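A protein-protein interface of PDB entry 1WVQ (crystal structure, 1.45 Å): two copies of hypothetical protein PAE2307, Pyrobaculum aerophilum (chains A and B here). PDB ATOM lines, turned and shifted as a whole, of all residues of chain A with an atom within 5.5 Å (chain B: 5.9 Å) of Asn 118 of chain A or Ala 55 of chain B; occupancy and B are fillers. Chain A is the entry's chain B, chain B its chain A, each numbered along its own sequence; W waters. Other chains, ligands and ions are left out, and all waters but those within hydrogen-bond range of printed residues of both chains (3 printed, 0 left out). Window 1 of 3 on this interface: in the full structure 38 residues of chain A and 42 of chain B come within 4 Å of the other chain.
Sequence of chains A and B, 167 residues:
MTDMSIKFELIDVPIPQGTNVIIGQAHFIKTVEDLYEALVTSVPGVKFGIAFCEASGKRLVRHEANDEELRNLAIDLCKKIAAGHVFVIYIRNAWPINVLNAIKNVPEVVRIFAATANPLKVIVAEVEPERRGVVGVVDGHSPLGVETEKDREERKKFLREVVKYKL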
ATOM      1  N   VAL A  13     -31.652 -14.448 -15.456  1.00  0.00           N
ATOM      2  CA  VAL A  13     -32.163 -13.096 -15.307  1.00  0.00           C
ATOM      3  C   VAL A  13     -31.199 -12.056 -15.858  1.00  0.00           C
ATOM      4  O   VAL A  13     -30.116 -11.844 -15.317  1.00  0.00           O
ATOM      5  CB  VAL A  13     -32.460 -12.770 -13.825  1.00  0.00           C
ATOM      6  CG1 VAL A  13     -33.021 -11.357 -13.707  1.00  0.00           C
ATOM      7  CG2 VAL A  13     -33.457 -13.769 -13.266  1.00  0.00           C
ATOM      8  N   ILE A  15     -29.461  -8.653 -16.361  1.00  0.00           N
ATOM      9  CA  ILE A  15     -29.347  -7.474 -15.509  1.00  0.00           C
ATOM     10  C   ILE A  15     -28.340  -6.503 -16.113  1.00  0.00           C
ATOM     11  O   ILE A  15     -27.137  -6.643 -15.906  1.00  0.00           O
ATOM     12  CB  ILE A  15     -28.899  -7.837 -14.077  1.00  0.00           C
ATOM     13  CG1 ILE A  15     -29.931  -8.762 -13.425  1.00  0.00           C
ATOM     14  CG2 ILE A  15     -28.757  -6.574 -13.239  1.00  0.00           C
ATOM     15  CD1 ILE A  15     -29.569  -9.196 -12.013  1.00  0.00           C
ATOM     16  N   THR A 116     -31.112  -7.826  -6.191  1.00  0.00           N
ATOM     17  CA  THR A 116     -29.697  -7.945  -6.498  1.00  0.00           C
ATOM     18  C   THR A 116     -29.317  -7.409  -7.871  1.00  0.00           C
ATOM     19  O   THR A 116     -30.174  -7.107  -8.701  1.00  0.00           O
ATOM     20  CB  THR A 116     -29.308  -9.447  -6.446  1.00  0.00           C
ATOM     21  OG1 THR A 116     -27.898  -9.604  -6.602  1.00  0.00           O
ATOM     22  CG2 THR A 116     -30.015 -10.215  -7.570  1.00  0.00           C
ATOM     23  N   ALA A 117     -28.009  -7.313  -8.093  1.00  0.00           N
ATOM     24  CA  ALA A 117     -27.469  -6.874  -9.370  1.00  0.00           C
ATOM     25  C   ALA A 117     -26.490  -7.950  -9.845  1.00  0.00           C
ATOM     26  O   ALA A 117     -25.806  -7.776 -10.847  1.00  0.00           O
ATOM     27  CB  ALA A 117     -26.752  -5.531  -9.211  1.00  0.00           C
ATOM     28  N   ASN A 118     -26.436  -9.066  -9.119  1.00  0.00           N
ATOM     29  CA  ASN A 118     -25.537 -10.176  -9.454  1.00  0.00           C
ATOM     30  C   ASN A 118     -26.129 -11.145 -10.453  1.00  0.00           C
ATOM     31  O   ASN A 118     -27.327 -11.114 -10.742  1.00  0.00           O
ATOM     32  CB  ASN A 118     -25.222 -11.048  -8.230  1.00  0.00           C
ATOM     33  CG  ASN A 118     -24.588 -10.296  -7.105  1.00  0.00           C
ATOM     34  OD1 ASN A 118     -23.693  -9.486  -7.306  1.00  0.00           O
ATOM     35  ND2 ASN A 118     -25.035 -10.583  -5.891  1.00  0.00           N
ATOM     36  N   PRO A 119     -25.281 -12.036 -10.991  1.00  0.00           N
ATOM     37  CA  PRO A 119     -25.756 -13.039 -11.940  1.00  0.00           C
ATOM     38  C   PRO A 119     -26.870 -13.708 -11.137  1.00  0.00           C
ATOM     39  O   PRO A 119     -26.693 -13.992  -9.946  1.00  0.00           O
ATOM     40  CB  PRO A 119     -24.545 -13.946 -12.098  1.00  0.00           C
ATOM     41  CG  PRO A 119     -23.415 -12.974 -12.042  1.00  0.00           C
ATOM     42  CD  PRO A 119     -23.806 -12.030 -10.921  1.00  0.00           C
ATOM     43  N   LEU A 120     -28.009 -13.956 -11.767  1.00  0.00           N
ATOM     44  CA  LEU A 120     -29.132 -14.524 -11.044  1.00  0.00           C
ATOM     45  C   LEU A 120     -29.926 -15.524 -11.866  1.00  0.00           C
ATOM     46  O   LEU A 120     -30.139 -15.329 -13.064  1.00  0.00           O
ATOM     47  CB  LEU A 120     -30.056 -13.383 -10.596  1.00  0.00           C
ATOM     48  CG  LEU A 120     -31.367 -13.700  -9.867  1.00  0.00           C
ATOM     49  CD1 LEU A 120     -31.084 -14.227  -8.462  1.00  0.00           C
ATOM     50  CD2 LEU A 120     -32.204 -12.426  -9.787  1.00  0.00           C
ATOM     51  N   ASP A 139     -28.651 -16.468  -6.253  1.00  0.00           N
ATOM     52  CA  ASP A 139     -28.168 -15.094  -6.256  1.00  0.00           C
ATOM     53  C   ASP A 139     -26.655 -15.011  -6.094  1.00  0.00           C
ATOM     54  O   ASP A 139     -26.128 -15.204  -5.008  1.00  0.00           O
ATOM     55  CB  ASP A 139     -28.870 -14.342  -5.121  1.00  0.00           C
ATOM     56  CG  ASP A 139     -28.586 -12.852  -5.129  1.00  0.00           C
ATOM     57  OD1 ASP A 139     -27.702 -12.400  -5.884  1.00  0.00           O
ATOM     58  OD2 ASP A 139     -29.252 -12.127  -4.360  1.00  0.00           O
ATOM     59  N   GLY A 140     -25.953 -14.715  -7.181  1.00  0.00           N
ATOM     60  CA  GLY A 140     -24.511 -14.623  -7.090  1.00  0.00           C
ATOM     61  C   GLY A 140     -23.836 -15.972  -6.924  1.00  0.00           C
ATOM     62  O   GLY A 140     -24.409 -17.012  -7.246  1.00  0.00           O
ATOM     63  N   HIS A 141     -22.621 -15.944  -6.381  1.00  0.00           N
ATOM     64  CA  HIS A 141     -21.817 -17.145  -6.209  1.00  0.00           C
ATOM     65  C   HIS A 141     -21.553 -17.538  -4.764  1.00  0.00           C
ATOM     66  O   HIS A 141     -21.751 -16.747  -3.845  1.00  0.00           O
ATOM     67  CB  HIS A 141     -20.479 -16.950  -6.926  1.00  0.00           C
ATOM     68  CG  HIS A 141     -20.612 -16.772  -8.403  1.00  0.00           C
ATOM     69  ND1 HIS A 141     -20.096 -17.673  -9.313  1.00  0.00           N
ATOM     70  CD2 HIS A 141     -21.214 -15.806  -9.134  1.00  0.00           C
ATOM     71  CE1 HIS A 141     -20.377 -17.266 -10.536  1.00  0.00           C
ATOM     72  NE2 HIS A 141     -21.055 -16.135 -10.457  1.00  0.00           N
ATOM     73  N   PHE B  52     -22.690 -13.661   6.992  1.00  0.00           N
ATOM     74  CA  PHE B  52     -23.373 -13.330   5.743  1.00  0.00           C
ATOM     75  C   PHE B  52     -22.529 -13.715   4.533  1.00  0.00           C
ATOM     76  O   PHE B  52     -21.340 -13.410   4.481  1.00  0.00           O
ATOM     77  CB  PHE B  52     -23.670 -11.827   5.717  1.00  0.00           C
ATOM     78  CG  PHE B  52     -24.139 -11.310   4.382  1.00  0.00           C
ATOM     79  CD1 PHE B  52     -25.374 -11.679   3.868  1.00  0.00           C
ATOM     80  CD2 PHE B  52     -23.355 -10.413   3.663  1.00  0.00           C
ATOM     81  CE1 PHE B  52     -25.826 -11.160   2.654  1.00  0.00           C
ATOM     82  CE2 PHE B  52     -23.795  -9.887   2.447  1.00  0.00           C
ATOM     83  CZ  PHE B  52     -25.033 -10.257   1.942  1.00  0.00           C
ATOM     84  N   CYS B  53     -23.150 -14.379   3.564  1.00  0.00           N
ATOM     85  CA  CYS B  53     -22.447 -14.799   2.356  1.00  0.00           C
ATOM     86  C   CYS B  53     -22.441 -13.723   1.274  1.00  0.00           C
ATOM     87  O   CYS B  53     -23.406 -13.581   0.528  1.00  0.00           O
ATOM     88  CB  CYS B  53     -23.081 -16.070   1.785  1.00  0.00           C
ATOM     89  SG  CYS B  53     -22.844 -17.536   2.806  1.00  0.00           S
ATOM     90  N   GLU B  54     -21.354 -12.961   1.203  1.00  0.00           N
ATOM     91  CA  GLU B  54     -21.205 -11.934   0.179  1.00  0.00           C
ATOM     92  C   GLU B  54     -21.181 -12.722  -1.131  1.00  0.00           C
ATOM     93  O   GLU B  54     -20.367 -13.628  -1.292  1.00  0.00           O
ATOM     94  CB  GLU B  54     -19.891 -11.180   0.400  1.00  0.00           C
ATOM     95  CG  GLU B  54     -19.506 -10.239  -0.719  1.00  0.00           C
ATOM     96  CD  GLU B  54     -18.195  -9.526  -0.443  1.00  0.00           C
ATOM     97  OE1 GLU B  54     -17.293 -10.142   0.160  1.00  0.00           O
ATOM     98  OE2 GLU B  54     -18.061  -8.352  -0.845  1.00  0.00           O
ATOM     99  N   ALA B  55     -22.068 -12.379  -2.062  1.00  0.00           N
ATOM    100  CA  ALA B  55     -22.177 -13.128  -3.312  1.00  0.00           C
ATOM    101  C   ALA B  55     -21.385 -12.637  -4.516  1.00  0.00           C
ATOM    102  O   ALA B  55     -21.424 -13.272  -5.572  1.00  0.00           O
ATOM    103  CB  ALA B  55     -23.645 -13.276  -3.690  1.00  0.00           C
ATOM    104  N   SER B  56     -20.687 -11.517  -4.365  1.00  0.00           N
ATOM    105  CA  SER B  56     -19.865 -10.967  -5.439  1.00  0.00           C
ATOM    106  C   SER B  56     -18.618 -10.368  -4.792  1.00  0.00           C
ATOM    107  O   SER B  56     -18.378 -10.581  -3.608  1.00  0.00           O
ATOM    108  CB  SER B  56     -20.640  -9.905  -6.231  1.00  0.00           C
ATOM    109  OG  SER B  56     -21.063  -8.835  -5.404  1.00  0.00           O
ATOM    110  N   GLY B  57     -17.821  -9.630  -5.555  1.00  0.00           N
ATOM    111  CA  GLY B  57     -16.614  -9.061  -4.981  1.00  0.00           C
ATOM    112  C   GLY B  57     -15.707 -10.165  -4.468  1.00  0.00           C
ATOM    113  O   GLY B  57     -15.472 -11.153  -5.164  1.00  0.00           O
ATOM    114  N   ARG B  59     -16.411 -12.240  -2.276  1.00  0.00           N
ATOM    115  CA  ARG B  59     -17.236 -13.399  -1.927  1.00  0.00           C
ATOM    116  C   ARG B  59     -16.842 -14.031  -0.599  1.00  0.00           C
ATOM    117  O   ARG B  59     -16.692 -15.250  -0.492  1.00  0.00           O
ATOM    118  CB  ARG B  59     -17.137 -14.451  -3.037  1.00  0.00           C
ATOM    119  CG  ARG B  59     -17.785 -14.018  -4.335  1.00  0.00           C
ATOM    120  CD  ARG B  59     -17.251 -14.821  -5.516  1.00  0.00           C
ATOM    121  NE  ARG B  59     -17.502 -16.255  -5.401  1.00  0.00           N
ATOM    122  CZ  ARG B  59     -17.108 -17.144  -6.305  1.00  0.00           C
ATOM    123  NH1 ARG B  59     -16.442 -16.737  -7.374  1.00  0.00           N
ATOM    124  NH2 ARG B  59     -17.395 -18.431  -6.154  1.00  0.00           N
ATOM    125  N   GLY B  84     -25.049 -17.737  -2.242  1.00  0.00           N
ATOM    126  CA  GLY B  84     -24.960 -16.293  -2.195  1.00  0.00           C
ATOM    127  C   GLY B  84     -26.070 -15.536  -1.494  1.00  0.00           C
ATOM    128  O   GLY B  84     -27.247 -15.817  -1.698  1.00  0.00           O
ATOM    129  N   NEP B  85     -25.674 -14.589  -0.652  1.00  0.00           N
ATOM    130  CA  NEP B  85     -26.596 -13.710   0.052  1.00  0.00           C
ATOM    131  C   NEP B  85     -27.408 -14.331   1.184  1.00  0.00           C
ATOM    132  O   NEP B  85     -28.379 -13.749   1.633  1.00  0.00           O
ATOM    133  CB  NEP B  85     -27.568 -13.086  -0.956  1.00  0.00           C
ATOM    134  CG  NEP B  85     -26.878 -11.958  -1.665  1.00  0.00           C
ATOM    135  ND1 NEP B  85     -27.448 -11.268  -2.703  1.00  0.00           N
ATOM    136  CD2 NEP B  85     -25.657 -11.409  -1.474  1.00  0.00           C
ATOM    137  CE1 NEP B  85     -26.594 -10.328  -3.129  1.00  0.00           C
ATOM    138  NE2 NEP B  85     -25.488 -10.409  -2.376  1.00  0.00           N
ATOM    139  P   NEP B  85     -24.022  -9.265  -2.648  1.00  0.00           P
ATOM    140  O1P NEP B  85     -23.091  -9.510  -1.502  1.00  0.00           O
ATOM    141  O2P NEP B  85     -24.434  -7.817  -2.699  1.00  0.00           O
ATOM    142  O3P NEP B  85     -23.340  -9.579  -3.930  1.00  0.00           O
HETATM  143  O   HOH W   1     -28.475 -17.699  -3.632  1.00  0.00           O
HETATM  144  O   HOH W   2     -21.354 -16.308  -1.126  1.00  0.00           O
HETATM  145  O   HOH W   3     -24.710 -18.791  -4.986  1.00  0.00           O
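The backbone NH (N) of His 141 of chain A lies within hydrogen-bond range of the backbone carbonyl oxygen (O) of Ala 55 of chain B (3.0 Å).
OG of Ser 56 of chain B sits close to OD1 of Asn 118 of chain A (3.3 Å).
ND1 of NEP 85 of chain B lies within hydrogen-bond range of the side-chain carboxylate of Asp 139 of chain A (2.6 Å).
ND2 of Asn 118 of chain A is in hydrogen-bond range of O3P of NEP 85 of chain B (2.8 Å).
O1P of NEP 85 of chain B lies within hydrogen-bond range of N of Ala 55 of chain B, at 3.1 Å.
The side-chain carboxylate of Asp 139 of chain A lies within hydrogen-bond range of the side-chain amide nitrogen of Asn 118 of chain A (3.2 Å).
OG1 of Thr 116 of chain A sits at hydrogen-bond distance from N of Asn 118 of chain A (3.0 Å).
The backbone carbonyl oxygen of Pro 119 of chain A lies within hydrogen-bond range of the backbone NH of Gly 140 of chain A, at 3.0 Å.
The side-chain hydroxyl of Ser 56 of chain B is in hydrogen-bond range of O3P of NEP 85 of chain B (2.8 Å).
The backbone NH (N) of Arg 59 of chain B is in hydrogen-bond range of the side-chain carboxylate (OE1) of Glu 54 of chain B (3.3 Å).
Thr 116 of chain A touches NEP 85 of chain B.
Asn 118 of chain A touches Ala 55 of chain B.
Asp 139 of chain A touches Ala 55 of chain B.
Asp 139 of chain A touches Gly 84 of chain B.
Gly 140 of chain A touches Ala 55 of chain B (CA to O, 3.7 Å).
Arg 59 of chain B touches His 141 of chain A (NE to CB, 3.4 Å).
His 141 of chain A touches Gly 84 of chain B (O to CA, 3.6 Å).
Of chain B, only Ala 55 (3.7 Å), Ser 56 (3.3 Å) and NEP 85 (2.8 Å) come within 4 Å of Asn 118 of chain A.
Of chain A, only Asn 118 (3.7 Å), Asp 139 (3.4 Å), Gly 140 (3.7 Å) and His 141 (3.0 Å) come within 4 Å of Ala 55 of chain B.
Printed residues of chain A within 4 Å of Ser 56 of chain B: Asn 118 (3.3 Å).
Of the printed residues of chain A, Arg 59 of chain B touches His 141.
Printed residues of chain A within 4 Å of Gly 84 of chain B: Asp 139 and His 141.
Of the printed residues of chain B, His 141 of chain A touches Ala 55 (3.0 Å), Arg 59 (3.4 Å) and Gly 84 (3.6 Å).
Of the printed residues of chain A, NEP 85 of chain B touches Thr 116 (3.8 Å), Asn 118 (2.8 Å) and Asp 139 (2.6 Å).
Phe 52 of chain B touches none of the printed residues of chain A.
The nearest printed residue of chain A that does not touch Ala 55 of chain B is Pro 119 of chain A (6.0 Å).
The nearest printed residue of chain A that does not touch Gly 84 of chain B is Gly 140 of chain A (4.9 Å).
Printed residues of chain B that touch a printed residue of chain A: Ala 55, Ser 56, Arg 59, Gly 84 and NEP 85.
Of the 10 printed residues of chain A, 5 touch a printed residue of chain B.
Among the printed residues, 11 pairs touch across the chains.
Among the printed residues, no Asp or Glu carboxylate lies within 4 Å of a Lys or Arg side-chain nitrogen of the other chain.
No position is printed for both chains.
Water W2 bridges O of His 141 of chain A (2.8 Å) and O of Glu 54 of chain B (2.9 Å).
Water W3 bridges O of Gly 140 of chain A (2.9 Å) and N of Gly 84 of chain B (3.0 Å).
Water W1 bridges the backbone NH of Asp 139 of chain A (2.9 Å) and the backbone carbonyl oxygen of Gly 84 of chain B (3.0 Å).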
